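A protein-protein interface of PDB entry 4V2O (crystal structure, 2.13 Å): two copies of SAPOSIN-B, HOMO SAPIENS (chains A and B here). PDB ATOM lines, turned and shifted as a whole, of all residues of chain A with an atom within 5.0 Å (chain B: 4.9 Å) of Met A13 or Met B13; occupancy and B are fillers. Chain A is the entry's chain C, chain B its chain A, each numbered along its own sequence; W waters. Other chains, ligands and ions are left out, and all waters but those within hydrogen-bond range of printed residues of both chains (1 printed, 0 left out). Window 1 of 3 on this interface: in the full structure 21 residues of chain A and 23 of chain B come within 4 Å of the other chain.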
ATOM      1  N   VAL A   6      12.167   5.500  -6.238  1.00  0.00           N
ATOM      2  CA  VAL A   6      11.180   4.410  -6.143  1.00  0.00           C
ATOM      3  C   VAL A   6      10.259   4.604  -4.935  1.00  0.00           C
ATOM      4  O   VAL A   6       9.044   4.422  -5.052  1.00  0.00           O
ATOM      5  CB  VAL A   6      11.863   3.017  -6.135  1.00  0.00           C
ATOM      6  CG1 VAL A   6      10.884   1.897  -5.766  1.00  0.00           C
ATOM      7  CG2 VAL A   6      12.552   2.741  -7.466  1.00  0.00           C
ATOM      8  N   ASP A   9       7.847   7.471  -5.594  1.00  0.00           N
ATOM      9  CA  ASP A   9       6.932   7.021  -6.644  1.00  0.00           C
ATOM     10  C   ASP A   9       5.843   6.139  -6.027  1.00  0.00           C
ATOM     11  O   ASP A   9       4.678   6.249  -6.400  1.00  0.00           O
ATOM     12  CB  ASP A   9       7.673   6.195  -7.683  1.00  0.00           C
ATOM     13  CG  ASP A   9       8.686   6.913  -8.544  1.00  0.00           C
ATOM     14  OD1 ASP A   9       8.657   8.161  -8.590  1.00  0.00           O
ATOM     15  OD2 ASP A   9       9.512   6.231  -9.151  1.00  0.00           O
ATOM     16  N   CYS A  10       6.246   5.249  -5.104  1.00  0.00           N
ATOM     17  CA  CYS A  10       5.352   4.342  -4.398  1.00  0.00           C
ATOM     18  C   CYS A  10       4.392   5.134  -3.518  1.00  0.00           C
ATOM     19  O   CYS A  10       3.190   4.861  -3.544  1.00  0.00           O
ATOM     20  CB  CYS A  10       6.142   3.315  -3.592  1.00  0.00           C
ATOM     21  SG  CYS A  10       5.112   2.116  -2.718  1.00  0.00           S
ATOM     22  N   ILE A  11       4.908   6.121  -2.757  1.00  0.00           N
ATOM     23  CA  ILE A  11       4.079   6.983  -1.900  1.00  0.00           C
ATOM     24  C   ILE A  11       3.001   7.670  -2.750  1.00  0.00           C
ATOM     25  O   ILE A  11       1.823   7.624  -2.386  1.00  0.00           O
ATOM     26  CB  ILE A  11       4.933   7.971  -1.053  1.00  0.00           C
ATOM     27  CG1 ILE A  11       5.750   7.196   0.017  1.00  0.00           C
ATOM     28  CG2 ILE A  11       4.051   9.076  -0.406  1.00  0.00           C
ATOM     29  CD1 ILE A  11       6.878   7.976   0.715  1.00  0.00           C
ATOM     30  N   GLN A  12       3.402   8.231  -3.910  1.00  0.00           N
ATOM     31  CA  GLN A  12       2.499   8.889  -4.857  1.00  0.00           C
ATOM     32  C   GLN A  12       1.437   7.906  -5.374  1.00  0.00           C
ATOM     33  O   GLN A  12       0.256   8.222  -5.325  1.00  0.00           O
ATOM     34  CB  GLN A  12       3.293   9.492  -6.027  1.00  0.00           C
ATOM     35  CG  GLN A  12       2.459  10.390  -6.942  1.00  0.00           C
ATOM     36  CD  GLN A  12       1.858  11.549  -6.180  1.00  0.00           C
ATOM     37  OE1 GLN A  12       2.569  12.340  -5.555  1.00  0.00           O
ATOM     38  NE2 GLN A  12       0.532  11.643  -6.167  1.00  0.00           N
ATOM     39  N   MET A  13       1.858   6.710  -5.836  1.00  0.00           N
ATOM     40  CA  MET A  13       0.949   5.682  -6.343  1.00  0.00           C
ATOM     41  C   MET A  13      -0.042   5.234  -5.280  1.00  0.00           C
ATOM     42  O   MET A  13      -1.230   5.183  -5.569  1.00  0.00           O
ATOM     43  CB  MET A  13       1.716   4.476  -6.893  1.00  0.00           C
ATOM     44  CG  MET A  13       0.825   3.460  -7.591  1.00  0.00           C
ATOM     45  SD  MET A  13       1.698   1.957  -8.076  1.00  0.00           S
ATOM     46  CE  MET A  13       1.935   1.179  -6.417  1.00  0.00           C
ATOM     47  N   VAL A  14       0.444   4.910  -4.065  1.00  0.00           N
ATOM     48  CA  VAL A  14      -0.389   4.448  -2.953  1.00  0.00           C
ATOM     49  C   VAL A  14      -1.410   5.510  -2.491  1.00  0.00           C
ATOM     50  O   VAL A  14      -2.557   5.153  -2.211  1.00  0.00           O
ATOM     51  CB  VAL A  14       0.417   3.773  -1.808  1.00  0.00           C
ATOM     52  CG1 VAL A  14      -0.502   3.366  -0.656  1.00  0.00           C
ATOM     53  CG2 VAL A  14       1.183   2.553  -2.323  1.00  0.00           C
ATOM     54  N   THR A  15      -1.016   6.806  -2.476  1.00  0.00           N
ATOM     55  CA  THR A  15      -1.900   7.926  -2.132  1.00  0.00           C
ATOM     56  C   THR A  15      -3.077   7.957  -3.120  1.00  0.00           C
ATOM     57  O   THR A  15      -4.226   8.058  -2.700  1.00  0.00           O
ATOM     58  CB  THR A  15      -1.122   9.261  -2.133  1.00  0.00           C
ATOM     59  OG1 THR A  15       0.007   9.150  -1.265  1.00  0.00           O
ATOM     60  CG2 THR A  15      -1.990  10.452  -1.699  1.00  0.00           C
ATOM     61  N   ASP A  16      -2.779   7.824  -4.427  1.00  0.00           N
ATOM     62  CA  ASP A  16      -3.778   7.813  -5.487  1.00  0.00           C
ATOM     63  C   ASP A  16      -4.654   6.557  -5.474  1.00  0.00           C
ATOM     64  O   ASP A  16      -5.830   6.658  -5.817  1.00  0.00           O
ATOM     65  CB  ASP A  16      -3.136   8.089  -6.859  1.00  0.00           C
ATOM     66  CG  ASP A  16      -2.607   9.515  -7.011  1.00  0.00           C
ATOM     67  OD1 ASP A  16      -3.089  10.414  -6.292  1.00  0.00           O
ATOM     68  OD2 ASP A  16      -1.738   9.735  -7.868  1.00  0.00           O
ATOM     69  N   ILE A  17      -4.103   5.393  -5.046  1.00  0.00           N
ATOM     70  CA  ILE A  17      -4.865   4.137  -4.899  1.00  0.00           C
ATOM     71  C   ILE A  17      -5.932   4.337  -3.815  1.00  0.00           C
ATOM     72  O   ILE A  17      -7.095   3.981  -4.021  1.00  0.00           O
ATOM     73  CB  ILE A  17      -3.957   2.904  -4.592  1.00  0.00           C
ATOM     74  CG1 ILE A  17      -3.114   2.513  -5.833  1.00  0.00           C
ATOM     75  CG2 ILE A  17      -4.793   1.699  -4.093  1.00  0.00           C
ATOM     76  CD1 ILE A  17      -1.920   1.609  -5.549  1.00  0.00           C
ATOM     77  N   PHE A  79       9.600  -0.916  -0.910  1.00  0.00           N
ATOM     78  CA  PHE A  79       9.950   0.190  -1.808  1.00  0.00           C
ATOM     79  C   PHE A  79      10.428   1.435  -1.064  1.00  0.00           C
ATOM     80  O   PHE A  79      11.105   2.268  -1.663  1.00  0.00           O
ATOM     81  CB  PHE A  79       8.833   0.488  -2.824  1.00  0.00           C
ATOM     82  CG  PHE A  79       8.510  -0.654  -3.764  1.00  0.00           C
ATOM     83  CD1 PHE A  79       9.521  -1.427  -4.322  1.00  0.00           C
ATOM     84  CD2 PHE A  79       7.197  -0.927  -4.129  1.00  0.00           C
ATOM     85  CE1 PHE A  79       9.220  -2.475  -5.201  1.00  0.00           C
ATOM     86  CE2 PHE A  79       6.898  -1.972  -5.010  1.00  0.00           C
ATOM     87  CZ  PHE A  79       7.913  -2.737  -5.540  1.00  0.00           C
ATOM     88  N   VAL B   6      -3.482   6.403 -11.104  1.00  0.00           N
ATOM     89  CA  VAL B   6      -2.852   5.176 -10.586  1.00  0.00           C
ATOM     90  C   VAL B   6      -1.993   4.495 -11.653  1.00  0.00           C
ATOM     91  O   VAL B   6      -0.869   4.079 -11.357  1.00  0.00           O
ATOM     92  CB  VAL B   6      -3.893   4.207  -9.961  1.00  0.00           C
ATOM     93  CG1 VAL B   6      -3.292   2.828  -9.670  1.00  0.00           C
ATOM     94  CG2 VAL B   6      -4.495   4.808  -8.698  1.00  0.00           C
ATOM     95  N   ASP B   9       1.153   6.541 -12.291  1.00  0.00           N
ATOM     96  CA  ASP B   9       1.978   6.449 -11.084  1.00  0.00           C
ATOM     97  C   ASP B   9       2.739   5.135 -11.101  1.00  0.00           C
ATOM     98  O   ASP B   9       3.912   5.108 -10.739  1.00  0.00           O
ATOM     99  CB  ASP B   9       1.103   6.463  -9.835  1.00  0.00           C
ATOM    100  CG  ASP B   9       0.395   7.745  -9.496  1.00  0.00           C
ATOM    101  OD1 ASP B   9       0.762   8.804 -10.062  1.00  0.00           O
ATOM    102  OD2 ASP B   9      -0.534   7.693  -8.685  1.00  0.00           O
ATOM    103  N   CYS B  10       2.059   4.045 -11.510  1.00  0.00           N
ATOM    104  CA  CYS B  10       2.638   2.717 -11.604  1.00  0.00           C
ATOM    105  C   CYS B  10       3.719   2.698 -12.694  1.00  0.00           C
ATOM    106  O   CYS B  10       4.803   2.180 -12.451  1.00  0.00           O
ATOM    107  CB  CYS B  10       1.554   1.673 -11.857  1.00  0.00           C
ATOM    108  SG  CYS B  10       2.184  -0.015 -11.982  1.00  0.00           S
ATOM    109  N   ILE B  11       3.431   3.277 -13.878  1.00  0.00           N
ATOM    110  CA  ILE B  11       4.399   3.360 -14.982  1.00  0.00           C
ATOM    111  C   ILE B  11       5.672   4.081 -14.502  1.00  0.00           C
ATOM    112  O   ILE B  11       6.770   3.563 -14.705  1.00  0.00           O
ATOM    113  CB  ILE B  11       3.776   3.973 -16.268  1.00  0.00           C
ATOM    114  CG1 ILE B  11       2.733   2.998 -16.883  1.00  0.00           C
ATOM    115  CG2 ILE B  11       4.874   4.353 -17.308  1.00  0.00           C
ATOM    116  CD1 ILE B  11       1.801   3.610 -17.957  1.00  0.00           C
ATOM    117  N   GLN B  12       5.505   5.226 -13.803  1.00  0.00           N
ATOM    118  CA  GLN B  12       6.597   6.012 -13.234  1.00  0.00           C
ATOM    119  C   GLN B  12       7.393   5.178 -12.223  1.00  0.00           C
ATOM    120  O   GLN B  12       8.613   5.114 -12.334  1.00  0.00           O
ATOM    121  CB  GLN B  12       6.053   7.288 -12.564  1.00  0.00           C
ATOM    122  CG  GLN B  12       7.131   8.285 -12.135  1.00  0.00           C
ATOM    123  CD  GLN B  12       7.973   8.723 -13.313  1.00  0.00           C
ATOM    124  OE1 GLN B  12       7.463   9.225 -14.313  1.00  0.00           O
ATOM    125  NE2 GLN B  12       9.272   8.469 -13.257  1.00  0.00           N
ATOM    126  N   MET B  13       6.711   4.522 -11.267  1.00  0.00           N
ATOM    127  CA  MET B  13       7.354   3.680 -10.251  1.00  0.00           C
ATOM    128  C   MET B  13       8.128   2.528 -10.879  1.00  0.00           C
ATOM    129  O   MET B  13       9.281   2.327 -10.510  1.00  0.00           O
ATOM    130  CB  MET B  13       6.339   3.139  -9.240  1.00  0.00           C
ATOM    131  CG  MET B  13       6.999   2.447  -8.056  1.00  0.00           C
ATOM    132  SD  MET B  13       5.832   1.660  -6.943  1.00  0.00           S
ATOM    133  CE  MET B  13       5.248   0.258  -8.032  1.00  0.00           C
ATOM    134  N   VAL B  14       7.501   1.787 -11.811  1.00  0.00           N
ATOM    135  CA  VAL B  14       8.116   0.645 -12.488  1.00  0.00           C
ATOM    136  C   VAL B  14       9.348   1.040 -13.328  1.00  0.00           C
ATOM    137  O   VAL B  14      10.351   0.328 -13.289  1.00  0.00           O
ATOM    138  CB  VAL B  14       7.094  -0.277 -13.209  1.00  0.00           C
ATOM    139  CG1 VAL B  14       7.805  -1.420 -13.937  1.00  0.00           C
ATOM    140  CG2 VAL B  14       6.075  -0.848 -12.220  1.00  0.00           C
ATOM    141  N   THR B  15       9.301   2.204 -14.013  1.00  0.00           N
ATOM    142  CA  THR B  15      10.430   2.746 -14.793  1.00  0.00           C
ATOM    143  C   THR B  15      11.630   2.968 -13.850  1.00  0.00           C
ATOM    144  O   THR B  15      12.749   2.564 -14.168  1.00  0.00           O
ATOM    145  CB  THR B  15      10.019   4.051 -15.512  1.00  0.00           C
ATOM    146  OG1 THR B  15       8.868   3.796 -16.322  1.00  0.00           O
ATOM    147  CG2 THR B  15      11.138   4.622 -16.382  1.00  0.00           C
ATOM    148  N   ASP B  16      11.379   3.582 -12.686  1.00  0.00           N
ATOM    149  CA  ASP B  16      12.399   3.848 -11.673  1.00  0.00           C
ATOM    150  C   ASP B  16      12.913   2.579 -10.986  1.00  0.00           C
ATOM    151  O   ASP B  16      14.087   2.538 -10.625  1.00  0.00           O
ATOM    152  CB  ASP B  16      11.929   4.920 -10.679  1.00  0.00           C
ATOM    153  CG  ASP B  16      11.800   6.313 -11.300  1.00  0.00           C
ATOM    154  OD1 ASP B  16      12.463   6.578 -12.332  1.00  0.00           O
ATOM    155  OD2 ASP B  16      11.078   7.146 -10.733  1.00  0.00           O
ATOM    156  N   ILE B  17      12.061   1.535 -10.833  1.00  0.00           N
ATOM    157  CA  ILE B  17      12.471   0.231 -10.271  1.00  0.00           C
ATOM    158  C   ILE B  17      13.493  -0.395 -11.222  1.00  0.00           C
ATOM    159  O   ILE B  17      14.532  -0.881 -10.770  1.00  0.00           O
ATOM    160  CB  ILE B  17      11.264  -0.726 -10.019  1.00  0.00           C
ATOM    161  CG1 ILE B  17      10.429  -0.248  -8.813  1.00  0.00           C
ATOM    162  CG2 ILE B  17      11.721  -2.204  -9.829  1.00  0.00           C
ATOM    163  CD1 ILE B  17       9.016  -0.852  -8.717  1.00  0.00           C
ATOM    164  N   PHE B  79      -3.084  -2.236 -12.395  1.00  0.00           N
ATOM    165  CA  PHE B  79      -3.067  -0.786 -12.201  1.00  0.00           C
ATOM    166  C   PHE B  79      -3.248   0.001 -13.498  1.00  0.00           C
ATOM    167  O   PHE B  79      -3.653   1.166 -13.444  1.00  0.00           O
ATOM    168  CB  PHE B  79      -1.845  -0.328 -11.378  1.00  0.00           C
ATOM    169  CG  PHE B  79      -1.788  -0.882  -9.968  1.00  0.00           C
ATOM    170  CD1 PHE B  79      -2.944  -0.984  -9.190  1.00  0.00           C
ATOM    171  CD2 PHE B  79      -0.578  -1.260  -9.401  1.00  0.00           C
ATOM    172  CE1 PHE B  79      -2.890  -1.496  -7.888  1.00  0.00           C
ATOM    173  CE2 PHE B  79      -0.522  -1.767  -8.098  1.00  0.00           C
ATOM    174  CZ  PHE B  79      -1.679  -1.881  -7.349  1.00  0.00           C
HETATM  175  O   HOH W   1       4.578   7.052  -8.951  1.00  0.00           O
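The side-chain carboxylate (OD2) of Asp B9 lies close to the side-chain carboxylate (OD2) of Asp A16. The side-chain carboxylate (OD2) of Asp A9 sits close to the side-chain carboxylate (OD2) of Asp B16 (2.4 Å). The backbone carbonyl oxygen (O) of Gln B12 lies close to the side-chain carboxylate (OD2) of Asp A9, 3.5 Å away. The side-chain carboxylate of Asp B9 lies close to the backbone carbonyl oxygen of Gln A12, at 3.5 Å.
The side-chain carboxylate (OD2) of Asp B16 lies within hydrogen-bond range of the side-chain amide nitrogen (NE2) of Gln B12 (3.4 Å). OD2 of Asp A16 lies within hydrogen-bond range of NE2 of Gln A12 (3.4 Å).
Asp B16 touches Val A6 (O to CG2, 3.5 Å). Val A6 touches Ile B17 (CG2 to N, 3.6 Å). OD2 of Asp A9 touches CA of Met B13, at 3.5 Å. Asp B9 touches Met A13. Met A13 touches Cys B10 (SD to CA, 3.7 Å). CE of Met A13 touches CE of Met B13 (3.8 Å). C of Asp A16 touches CG2 of Val B6 (3.7 Å). CG2 of Val B6 touches N of Ile A17, 3.7 Å away. CD1 of Ile A17 touches CZ of Phe B79, at 3.9 Å. CZ of Phe A79 touches CD1 of Ile B17, 3.9 Å away.
Printed residues of chain B within 4 Å of Asp A9: Gln B12 (3.5 Å), Met B13 (3.5 Å) and Asp B16 (2.4 Å). Of chain B, only Asp B9, Cys B10 and Met B13 come within 4 Å of Met A13. Of the printed residues of chain B, Asp A16 touches Val B6 (3.7 Å) and Asp B9 (2.5 Å). Of the printed residues of chain B, Ile A17 touches Val B6 and Phe B79. Of the printed residues of chain B, Phe A79 touches Ile B17 (3.9 Å). Ile B11 touches none of the printed residues of chain A. Met B13 touches just these residues of chain A: Asp A9, Cys A10 and Met A13. Val B14 touches none of the printed residues of chain A. Of the printed residues of chain A, Phe B79 touches Ile A17 (3.9 Å). The nearest residue of chain A that does not touch Met B13 is Phe A79 (4.1 Å). The nearest printed residue of chain B that does not touch Asp A16 is Cys B10 (7.7 Å).
Printed residues of chain B that touch a printed residue of chain A: Val B6, Asp B9, Cys B10, Gln B12, Met B13, Asp B16, Ile B17 and Phe B79. Hydrophobic or aromatic side chains of chain B that line the printed part of chain A: Val B6, Met B13, Ile B17 and Phe B79. Hydrophobic or aromatic side chains of chain A within 4 Å of the printed part of chain B: Val A6, Met A13, Ile A17 and Phe A79. Among the printed residues, 15 pairs touch across the chains. Among the printed residues, no Asp or Glu carboxylate lies within 4 Å of a Lys or Arg side-chain nitrogen of the other chain.
Val A6 touches Asp B16, and with the chains exchanged Asp A16 touches Val B6. Asp A9 touches Gln B12, and with the chains exchanged Gln A12 touches Asp B9. Asp A9 touches Asp B16, and with the chains exchanged Asp A16 touches Asp B9. Ile A17 touches Phe B79, and with the chains exchanged Phe A79 touches Ile B17. 11 positions are printed for both chains.
Water W1 lies within hydrogen-bond range of O of Asp A9 and O of Asp B9.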
